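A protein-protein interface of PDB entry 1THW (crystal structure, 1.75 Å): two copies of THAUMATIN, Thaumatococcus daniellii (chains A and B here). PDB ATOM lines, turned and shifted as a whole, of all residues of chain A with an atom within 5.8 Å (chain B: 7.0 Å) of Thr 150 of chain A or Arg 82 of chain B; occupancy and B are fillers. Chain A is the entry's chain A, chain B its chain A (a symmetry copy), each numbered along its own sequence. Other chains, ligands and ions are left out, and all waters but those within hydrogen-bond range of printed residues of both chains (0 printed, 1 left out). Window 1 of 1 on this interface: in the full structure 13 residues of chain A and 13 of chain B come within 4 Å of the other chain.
Of chain B, only Arg 82 comes within 4 Å of Thr 150 of chain A.
Of the printed residues of chain B, Phe 152 of chain A touches Pro 141.
Printed residues of chain A within 4 Å of Ile 65 of chain B: Gln 153.
Of the printed residues of chain A, Cys 66 of chain B touches Gln 153 (3.5 Å).
Arg 82 of chain B touches two residues of chain A.
Of the printed residues of chain A, Pro 141 of chain B touches Val 151 and Phe 152.
The nearest residue of chain B that does not touch Thr 150 of chain A is Pro 141 of chain B (6.9 Å).
Among the printed residues, pairs that only touch across the chains: Gln 153 of chain A with Arg 82 of chain B, Gln 153 of chain A with Lys 67 of chain B, Val 151 of chain A with Pro 141 of chain B, Phe 152 of chain A with Pro 141 of chain B and Gln 153 of chain A with Ile 65 of chain B.
Of the 21 printed residues of chain B, 5 touch a printed residue of chain A.
Printed residues of chain B that touch a printed residue of chain A: Ile 65, Cys 66, Lys 67, Arg 82 and Pro 141.
Along chain B the printed residues that touch a printed residue of chain A span positions 65 to 141.
Of the 12 printed residues of chain A, 4 touch a printed residue of chain B.
Hydrophobic or aromatic side chains of chain A that line the printed part of chain B: Val 151 and Phe 152.
Among the printed residues, 7 pairs touch across the chains.
The backbone carbonyl oxygen (O) of Cys 66 of chain B lies close to the side-chain amide oxygen (OE1) of Gln 153 of chain A (3.5 Å).
NH2 of Arg 82 of chain B sits at hydrogen-bond distance from O of Thr 150 of chain A (2.9 Å).
Positions printed for both chains: 83, 106, 146 and 150.
Of the 7 pairs that touch across the chains among the printed residues, none has its exchanged pair printed and touching as well.
The side-chain carboxylate of Asp 70 of chain B sits at hydrogen-bond distance from the backbone NH of Cys 66 of chain B.
O of Arg 82 of chain B is in hydrogen-bond range of N of Gly 69 of chain B.
The side-chain carboxylate (OD1) of Asp 147 of chain A is in hydrogen-bond range of the side-chain hydroxyl (OG1) of Thr 150 of chain A, at 2.6 Å.
The side-chain amide nitrogen (NE2) of Gln 153 of chain A is in hydrogen-bond range of the backbone carbonyl oxygen (O) of Cys 149 of chain A.
The side-chain sulfur of Cys 158 of chain A is disulfide-bonded to the side-chain sulfur of Cys 149 of chain A, at 2.1 Å.
The backbone NH of Arg 82 of chain B sits at hydrogen-bond distance from the backbone carbonyl oxygen of Asp 70 of chain B (2.8 Å).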
ATOM      1  N   PRO A  83       1.955  22.352  15.010  1.00  0.00           N
ATOM      2  CA  PRO A  83       1.009  23.314  14.475  1.00  0.00           C
ATOM      3  C   PRO A  83      -0.275  22.612  14.085  1.00  0.00           C
ATOM      4  O   PRO A  83      -0.251  21.407  13.817  1.00  0.00           O
ATOM      5  CB  PRO A  83       1.655  23.952  13.247  1.00  0.00           C
ATOM      6  CG  PRO A  83       3.134  23.640  13.465  1.00  0.00           C
ATOM      7  CD  PRO A  83       3.240  22.368  14.306  1.00  0.00           C
ATOM      8  N   ILE A 105       2.721  32.544  13.056  1.00  0.00           N
ATOM      9  CA  ILE A 105       3.773  31.891  12.230  1.00  0.00           C
ATOM     10  C   ILE A 105       3.634  30.359  12.159  1.00  0.00           C
ATOM     11  O   ILE A 105       3.986  29.722  11.140  1.00  0.00           O
ATOM     12  CB  ILE A 105       5.207  32.335  12.633  1.00  0.00           C
ATOM     13  CG1 ILE A 105       5.317  33.793  12.169  1.00  0.00           C
ATOM     14  CG2 ILE A 105       6.316  31.556  11.892  1.00  0.00           C
ATOM     15  CD1 ILE A 105       6.628  34.458  12.645  1.00  0.00           C
ATOM     16  N   LYS A 106       3.074  29.782  13.214  1.00  0.00           N
ATOM     17  CA  LYS A 106       2.848  28.351  13.285  1.00  0.00           C
ATOM     18  C   LYS A 106       1.358  28.076  13.202  1.00  0.00           C
ATOM     19  O   LYS A 106       0.956  27.013  13.716  1.00  0.00           O
ATOM     20  CB  LYS A 106       3.277  27.754  14.625  1.00  0.00           C
ATOM     21  CG  LYS A 106       4.734  28.001  14.972  1.00  0.00           C
ATOM     22  CD  LYS A 106       5.539  27.291  13.952  1.00  0.00           C
ATOM     23  CE  LYS A 106       7.032  27.134  14.204  1.00  0.00           C
ATOM     24  NZ  LYS A 106       7.644  26.369  13.092  1.00  0.00           N
ATOM     25  N   ASN A 146      -3.554  25.975   9.480  1.00  0.00           N
ATOM     26  CA  ASN A 146      -2.112  25.936   9.436  1.00  0.00           C
ATOM     27  C   ASN A 146      -1.508  27.124   8.729  1.00  0.00           C
ATOM     28  O   ASN A 146      -2.136  27.777   7.883  1.00  0.00           O
ATOM     29  CB  ASN A 146      -1.730  24.736   8.514  1.00  0.00           C
ATOM     30  CG  ASN A 146      -1.732  23.413   9.271  1.00  0.00           C
ATOM     31  OD1 ASN A 146      -1.230  23.319  10.413  1.00  0.00           O
ATOM     32  ND2 ASN A 146      -2.374  22.430   8.623  1.00  0.00           N
ATOM     33  N   ASP A 147      -0.223  27.352   9.008  1.00  0.00           N
ATOM     34  CA  ASP A 147       0.502  28.383   8.247  1.00  0.00           C
ATOM     35  C   ASP A 147       1.031  27.687   6.972  1.00  0.00           C
ATOM     36  O   ASP A 147       1.118  26.426   6.885  1.00  0.00           O
ATOM     37  CB  ASP A 147       1.711  28.829   9.048  1.00  0.00           C
ATOM     38  CG  ASP A 147       2.596  27.667   9.358  1.00  0.00           C
ATOM     39  OD1 ASP A 147       2.296  26.843  10.164  1.00  0.00           O
ATOM     40  OD2 ASP A 147       3.718  27.591   8.648  1.00  0.00           O
ATOM     41  N   ALA A 148       1.372  28.517   5.973  1.00  0.00           N
ATOM     42  CA  ALA A 148       1.822  27.987   4.666  1.00  0.00           C
ATOM     43  C   ALA A 148       3.153  27.234   4.683  1.00  0.00           C
ATOM     44  O   ALA A 148       3.426  26.394   3.806  1.00  0.00           O
ATOM     45  CB  ALA A 148       1.954  29.181   3.682  1.00  0.00           C
ATOM     46  N   CYS A 149       4.022  27.561   5.598  1.00  0.00           N
ATOM     47  CA  CYS A 149       5.307  26.852   5.670  1.00  0.00           C
ATOM     48  C   CYS A 149       5.055  25.436   6.084  1.00  0.00           C
ATOM     49  O   CYS A 149       5.510  24.460   5.459  1.00  0.00           O
ATOM     50  CB  CYS A 149       6.228  27.551   6.674  1.00  0.00           C
ATOM     51  SG  CYS A 149       7.758  26.625   7.115  1.00  0.00           S
ATOM     52  N   THR A 150       4.259  25.276   7.164  1.00  0.00           N
ATOM     53  CA  THR A 150       3.913  23.879   7.564  1.00  0.00           C
ATOM     54  C   THR A 150       3.279  23.078   6.437  1.00  0.00           C
ATOM     55  O   THR A 150       3.626  21.955   6.211  1.00  0.00           O
ATOM     56  CB  THR A 150       2.860  23.924   8.708  1.00  0.00           C
ATOM     57  OG1 THR A 150       3.459  24.563   9.774  1.00  0.00           O
ATOM     58  CG2 THR A 150       2.502  22.517   9.127  1.00  0.00           C
ATOM     59  N   VAL A 151       2.345  23.633   5.657  1.00  0.00           N
ATOM     60  CA  VAL A 151       1.731  22.883   4.639  1.00  0.00           C
ATOM     61  C   VAL A 151       2.642  22.621   3.445  1.00  0.00           C
ATOM     62  O   VAL A 151       2.702  21.494   2.984  1.00  0.00           O
ATOM     63  CB  VAL A 151       0.495  23.656   4.170  1.00  0.00           C
ATOM     64  CG1 VAL A 151      -0.230  22.948   3.011  1.00  0.00           C
ATOM     65  CG2 VAL A 151      -0.502  23.915   5.330  1.00  0.00           C
ATOM     66  N   PHE A 152       3.260  23.699   2.899  1.00  0.00           N
ATOM     67  CA  PHE A 152       3.972  23.605   1.572  1.00  0.00           C
ATOM     68  C   PHE A 152       5.474  23.343   1.613  1.00  0.00           C
ATOM     69  O   PHE A 152       6.093  22.952   0.619  1.00  0.00           O
ATOM     70  CB  PHE A 152       3.625  24.857   0.727  1.00  0.00           C
ATOM     71  CG  PHE A 152       2.154  24.882   0.388  1.00  0.00           C
ATOM     72  CD1 PHE A 152       1.633  23.977  -0.546  1.00  0.00           C
ATOM     73  CD2 PHE A 152       1.331  25.829   1.002  1.00  0.00           C
ATOM     74  CE1 PHE A 152       0.271  23.997  -0.865  1.00  0.00           C
ATOM     75  CE2 PHE A 152      -0.017  25.879   0.667  1.00  0.00           C
ATOM     76  CZ  PHE A 152      -0.550  24.953  -0.235  1.00  0.00           C
ATOM     77  N   GLN A 153       6.087  23.659   2.722  1.00  0.00           N
ATOM     78  CA  GLN A 153       7.496  23.409   2.922  1.00  0.00           C
ATOM     79  C   GLN A 153       8.380  24.020   1.835  1.00  0.00           C
ATOM     80  O   GLN A 153       9.278  23.323   1.346  1.00  0.00           O
ATOM     81  CB  GLN A 153       7.754  21.891   2.991  1.00  0.00           C
ATOM     82  CG  GLN A 153       7.115  21.152   4.240  1.00  0.00           C
ATOM     83  CD  GLN A 153       7.937  21.392   5.521  1.00  0.00           C
ATOM     84  OE1 GLN A 153       8.869  20.652   5.841  1.00  0.00           O
ATOM     85  NE2 GLN A 153       7.643  22.455   6.302  1.00  0.00           N
ATOM     86  N   CYS A 158       8.770  29.462   4.308  1.00  0.00           N
ATOM     87  CA  CYS A 158       9.558  29.168   5.497  1.00  0.00           C
ATOM     88  C   CYS A 158      10.663  30.170   5.732  1.00  0.00           C
ATOM     89  O   CYS A 158      11.241  30.190   6.826  1.00  0.00           O
ATOM     90  CB  CYS A 158      10.074  27.672   5.576  1.00  0.00           C
ATOM     91  SG  CYS A 158       8.760  26.452   5.329  1.00  0.00           S
ATOM     92  N   TRP B  51      16.106   7.049   5.304  1.00  0.00           N
ATOM     93  CA  TRP B  51      15.000   7.481   4.474  1.00  0.00           C
ATOM     94  C   TRP B  51      15.572   8.458   3.438  1.00  0.00           C
ATOM     95  O   TRP B  51      16.761   8.853   3.553  1.00  0.00           O
ATOM     96  CB  TRP B  51      13.916   8.262   5.274  1.00  0.00           C
ATOM     97  CG  TRP B  51      14.307   9.565   5.974  1.00  0.00           C
ATOM     98  CD1 TRP B  51      13.933  10.797   5.602  1.00  0.00           C
ATOM     99  CD2 TRP B  51      14.996   9.752   7.237  1.00  0.00           C
ATOM    100  NE1 TRP B  51      14.405  11.756   6.485  1.00  0.00           N
ATOM    101  CE2 TRP B  51      15.010  11.125   7.514  1.00  0.00           C
ATOM    102  CE3 TRP B  51      15.659   8.852   8.121  1.00  0.00           C
ATOM    103  CZ2 TRP B  51      15.702  11.640   8.587  1.00  0.00           C
ATOM    104  CZ3 TRP B  51      16.336   9.351   9.220  1.00  0.00           C
ATOM    105  CH2 TRP B  51      16.314  10.731   9.462  1.00  0.00           C
ATOM    106  N   ALA B  52      14.701   8.821   2.469  1.00  0.00           N
ATOM    107  CA  ALA B  52      15.062   9.793   1.456  1.00  0.00           C
ATOM    108  C   ALA B  52      14.295  11.016   1.726  1.00  0.00           C
ATOM    109  O   ALA B  52      13.155  10.957   2.280  1.00  0.00           O
ATOM    110  CB  ALA B  52      14.689   9.269   0.061  1.00  0.00           C
ATOM    111  N   ILE B  65      15.790  23.362   3.657  1.00  0.00           N
ATOM    112  CA  ILE B  65      14.447  22.786   3.797  1.00  0.00           C
ATOM    113  C   ILE B  65      14.264  21.683   2.720  1.00  0.00           C
ATOM    114  O   ILE B  65      14.908  21.686   1.663  1.00  0.00           O
ATOM    115  CB  ILE B  65      13.427  23.939   3.674  1.00  0.00           C
ATOM    116  CG1 ILE B  65      11.985  23.650   4.012  1.00  0.00           C
ATOM    117  CG2 ILE B  65      13.515  24.552   2.279  1.00  0.00           C
ATOM    118  CD1 ILE B  65      11.898  22.936   5.327  1.00  0.00           C
ATOM    119  N   CYS B  66      13.366  20.717   2.984  1.00  0.00           N
ATOM    120  CA  CYS B  66      13.039  19.650   2.046  1.00  0.00           C
ATOM    121  C   CYS B  66      11.530  19.519   2.138  1.00  0.00           C
ATOM    122  O   CYS B  66      10.996  19.758   3.244  1.00  0.00           O
ATOM    123  CB  CYS B  66      13.621  18.274   2.499  1.00  0.00           C
ATOM    124  SG  CYS B  66      15.443  18.206   2.519  1.00  0.00           S
ATOM    125  N   LYS B  67      10.873  19.175   1.004  1.00  0.00           N
ATOM    126  CA  LYS B  67       9.448  19.032   0.987  1.00  0.00           C
ATOM    127  C   LYS B  67       8.999  17.740   1.666  1.00  0.00           C
ATOM    128  O   LYS B  67       7.912  17.705   2.226  1.00  0.00           O
ATOM    129  CB  LYS B  67       8.907  19.213  -0.390  1.00  0.00           C
ATOM    130  CG  LYS B  67       9.269  20.549  -0.977  1.00  0.00           C
ATOM    131  CD  LYS B  67       8.135  20.589  -1.926  1.00  0.00           C
ATOM    132  CE  LYS B  67       8.387  21.361  -3.156  1.00  0.00           C
ATOM    133  NZ  LYS B  67       8.628  22.707  -2.741  1.00  0.00           N
ATOM    134  N   THR B  68       9.822  16.698   1.664  1.00  0.00           N
ATOM    135  CA  THR B  68       9.468  15.469   2.401  1.00  0.00           C
ATOM    136  C   THR B  68      10.679  15.072   3.223  1.00  0.00           C
ATOM    137  O   THR B  68      11.805  15.309   2.796  1.00  0.00           O
ATOM    138  CB  THR B  68       9.015  14.235   1.555  1.00  0.00           C
ATOM    139  OG1 THR B  68      10.088  13.789   0.696  1.00  0.00           O
ATOM    140  CG2 THR B  68       7.816  14.635   0.714  1.00  0.00           C
ATOM    141  N   GLY B  69      10.455  14.527   4.430  1.00  0.00           N
ATOM    142  CA  GLY B  69      11.485  14.023   5.330  1.00  0.00           C
ATOM    143  C   GLY B  69      12.447  15.045   5.913  1.00  0.00           C
ATOM    144  O   GLY B  69      13.473  14.678   6.390  1.00  0.00           O
ATOM    145  N   ASP B  70      12.110  16.301   5.998  1.00  0.00           N
ATOM    146  CA  ASP B  70      13.065  17.293   6.536  1.00  0.00           C
ATOM    147  C   ASP B  70      13.377  16.995   7.975  1.00  0.00           C
ATOM    148  O   ASP B  70      12.426  16.679   8.705  1.00  0.00           O
ATOM    149  CB  ASP B  70      12.434  18.668   6.466  1.00  0.00           C
ATOM    150  CG  ASP B  70      13.318  19.821   6.904  1.00  0.00           C
ATOM    151  OD1 ASP B  70      14.324  20.063   6.142  1.00  0.00           O
ATOM    152  OD2 ASP B  70      13.120  20.431   7.909  1.00  0.00           O
ATOM    153  N   CYS B  71      14.660  17.077   8.380  1.00  0.00           N
ATOM    154  CA  CYS B  71      15.058  16.775   9.753  1.00  0.00           C
ATOM    155  C   CYS B  71      15.534  18.037  10.395  1.00  0.00           C
ATOM    156  O   CYS B  71      16.666  18.331  10.506  1.00  0.00           O
ATOM    157  CB  CYS B  71      16.125  15.708   9.865  1.00  0.00           C
ATOM    158  SG  CYS B  71      17.595  16.212   8.926  1.00  0.00           S
ATOM    159  N   GLY B  72      14.627  18.897  10.697  1.00  0.00           N
ATOM    160  CA  GLY B  72      15.031  20.152  11.271  1.00  0.00           C
ATOM    161  C   GLY B  72      15.790  21.057  10.323  1.00  0.00           C
ATOM    162  O   GLY B  72      16.571  21.808  10.826  1.00  0.00           O
ATOM    163  N   PHE B  80      14.974  12.389  13.509  1.00  0.00           N
ATOM    164  CA  PHE B  80      14.124  11.826  12.442  1.00  0.00           C
ATOM    165  C   PHE B  80      13.477  12.937  11.594  1.00  0.00           C
ATOM    166  O   PHE B  80      13.368  14.117  11.995  1.00  0.00           O
ATOM    167  CB  PHE B  80      13.140  10.806  13.003  1.00  0.00           C
ATOM    168  CG  PHE B  80      13.835   9.667  13.698  1.00  0.00           C
ATOM    169  CD1 PHE B  80      14.886   8.965  13.101  1.00  0.00           C
ATOM    170  CD2 PHE B  80      13.370   9.183  14.918  1.00  0.00           C
ATOM    171  CE1 PHE B  80      15.506   7.859  13.671  1.00  0.00           C
ATOM    172  CE2 PHE B  80      13.958   8.066  15.519  1.00  0.00           C
ATOM    173  CZ  PHE B  80      15.033   7.421  14.902  1.00  0.00           C
ATOM    174  N   GLY B  81      13.049  12.575  10.393  1.00  0.00           N
ATOM    175  CA  GLY B  81      12.448  13.528   9.452  1.00  0.00           C
ATOM    176  C   GLY B  81      10.922  13.614   9.556  1.00  0.00           C
ATOM    177  O   GLY B  81      10.213  12.713  10.033  1.00  0.00           O
ATOM    178  N   ARG B  82      10.440  14.709   9.055  1.00  0.00           N
ATOM    179  CA  ARG B  82       9.029  14.982   9.012  1.00  0.00           C
ATOM    180  C   ARG B  82       8.340  14.118   7.942  1.00  0.00           C
ATOM    181  O   ARG B  82       8.815  14.016   6.806  1.00  0.00           O
ATOM    182  CB  ARG B  82       8.923  16.500   8.728  1.00  0.00           C
ATOM    183  CG  ARG B  82       7.506  17.027   8.557  1.00  0.00           C
ATOM    184  CD  ARG B  82       7.537  18.521   8.296  1.00  0.00           C
ATOM    185  NE  ARG B  82       6.216  19.049   8.548  1.00  0.00           N
ATOM    186  CZ  ARG B  82       5.315  19.324   7.606  1.00  0.00           C
ATOM    187  NH1 ARG B  82       5.542  19.156   6.301  1.00  0.00           N
ATOM    188  NH2 ARG B  82       4.124  19.739   7.994  1.00  0.00           N
ATOM    189  N   PRO B  83       7.190  13.502   8.265  1.00  0.00           N
ATOM    190  CA  PRO B  83       6.463  12.684   7.313  1.00  0.00           C
ATOM    191  C   PRO B  83       5.998  13.535   6.149  1.00  0.00           C
ATOM    192  O   PRO B  83       5.851  14.750   6.308  1.00  0.00           O
ATOM    193  CB  PRO B  83       5.260  12.093   8.047  1.00  0.00           C
ATOM    194  CG  PRO B  83       5.673  12.243   9.510  1.00  0.00           C
ATOM    195  CD  PRO B  83       6.639  13.424   9.620  1.00  0.00           C
ATOM    196  N   PRO B  84       5.716  12.945   5.007  1.00  0.00           N
ATOM    197  CA  PRO B  84       5.724  11.529   4.799  1.00  0.00           C
ATOM    198  C   PRO B  84       7.102  11.035   4.466  1.00  0.00           C
ATOM    199  O   PRO B  84       7.799  11.674   3.673  1.00  0.00           O
ATOM    200  CB  PRO B  84       4.806  11.310   3.578  1.00  0.00           C
ATOM    201  CG  PRO B  84       4.696  12.669   2.844  1.00  0.00           C
ATOM    202  CD  PRO B  84       5.321  13.677   3.764  1.00  0.00           C
ATOM    203  N   THR B  85       7.458   9.874   4.962  1.00  0.00           N
ATOM    204  CA  THR B  85       8.765   9.258   4.695  1.00  0.00           C
ATOM    205  C   THR B  85       8.682   7.753   4.724  1.00  0.00           C
ATOM    206  O   THR B  85       8.402   7.165   5.774  1.00  0.00           O
ATOM    207  CB  THR B  85       9.846   9.528   5.795  1.00  0.00           C
ATOM    208  OG1 THR B  85       9.285   9.188   7.050  1.00  0.00           O
ATOM    209  CG2 THR B  85      10.293  10.967   5.877  1.00  0.00           C
ATOM    210  N   LYS B 106       4.834   6.178   8.962  1.00  0.00           N
ATOM    211  CA  LYS B 106       5.015   7.614   8.851  1.00  0.00           C
ATOM    212  C   LYS B 106       4.790   8.035   7.410  1.00  0.00           C
ATOM    213  O   LYS B 106       5.354   9.084   7.039  1.00  0.00           O
ATOM    214  CB  LYS B 106       6.445   8.051   9.162  1.00  0.00           C
ATOM    215  CG  LYS B 106       6.930   7.639  10.541  1.00  0.00           C
ATOM    216  CD  LYS B 106       6.081   8.353  11.520  1.00  0.00           C
ATOM    217  CE  LYS B 106       6.513   8.345  12.979  1.00  0.00           C
ATOM    218  NZ  LYS B 106       5.556   9.140  13.784  1.00  0.00           N
ATOM    219  N   ASN B 109       7.041   8.324   0.775  1.00  0.00           N
ATOM    220  CA  ASN B 109       7.481   9.324  -0.179  1.00  0.00           C
ATOM    221  C   ASN B 109       8.209   8.727  -1.395  1.00  0.00           C
ATOM    222  O   ASN B 109       7.896   9.156  -2.540  1.00  0.00           O
ATOM    223  CB  ASN B 109       8.269  10.469   0.437  1.00  0.00           C
ATOM    224  CG  ASN B 109       9.594   9.992   1.074  1.00  0.00           C
ATOM    225  OD1 ASN B 109      10.520  10.819   1.191  1.00  0.00           O
ATOM    226  ND2 ASN B 109       9.742   8.740   1.418  1.00  0.00           N
ATOM    227  N   PRO B 141       0.719  18.037  -0.024  1.00  0.00           N
ATOM    228  CA  PRO B 141       0.963  19.053  -1.038  1.00  0.00           C
ATOM    229  C   PRO B 141       2.375  19.037  -1.537  1.00  0.00           C
ATOM    230  O   PRO B 141       2.574  18.960  -2.754  1.00  0.00           O
ATOM    231  CB  PRO B 141       0.675  20.373  -0.362  1.00  0.00           C
ATOM    232  CG  PRO B 141      -0.198  20.031   0.843  1.00  0.00           C
ATOM    233  CD  PRO B 141       0.099  18.591   1.199  1.00  0.00           C
ATOM    234  N   ASN B 146       0.752  10.901   3.181  1.00  0.00           N
ATOM    235  CA  ASN B 146       0.876  10.806   4.617  1.00  0.00           C
ATOM    236  C   ASN B 146       0.132   9.630   5.199  1.00  0.00           C
ATOM    237  O   ASN B 146      -0.838   9.114   4.625  1.00  0.00           O
ATOM    238  CB  ASN B 146       0.122  12.038   5.208  1.00  0.00           C
ATOM    239  CG  ASN B 146       0.996  13.287   5.226  1.00  0.00           C
ATOM    240  OD1 ASN B 146       2.191  13.235   5.591  1.00  0.00           O
ATOM    241  ND2 ASN B 146       0.376  14.378   4.752  1.00  0.00           N
ATOM    242  N   THR B 150      -0.586  11.047  11.249  1.00  0.00           N
ATOM    243  CA  THR B 150      -0.097  12.431  10.977  1.00  0.00           C
ATOM    244  C   THR B 150      -1.208  13.382  10.554  1.00  0.00           C
ATOM    245  O   THR B 150      -1.284  14.481  11.019  1.00  0.00           O
ATOM    246  CB  THR B 150       0.911  12.390   9.793  1.00  0.00           C
ATOM    247  OG1 THR B 150       1.972  11.609  10.202  1.00  0.00           O
ATOM    248  CG2 THR B 150       1.418  13.784   9.507  1.00  0.00           C
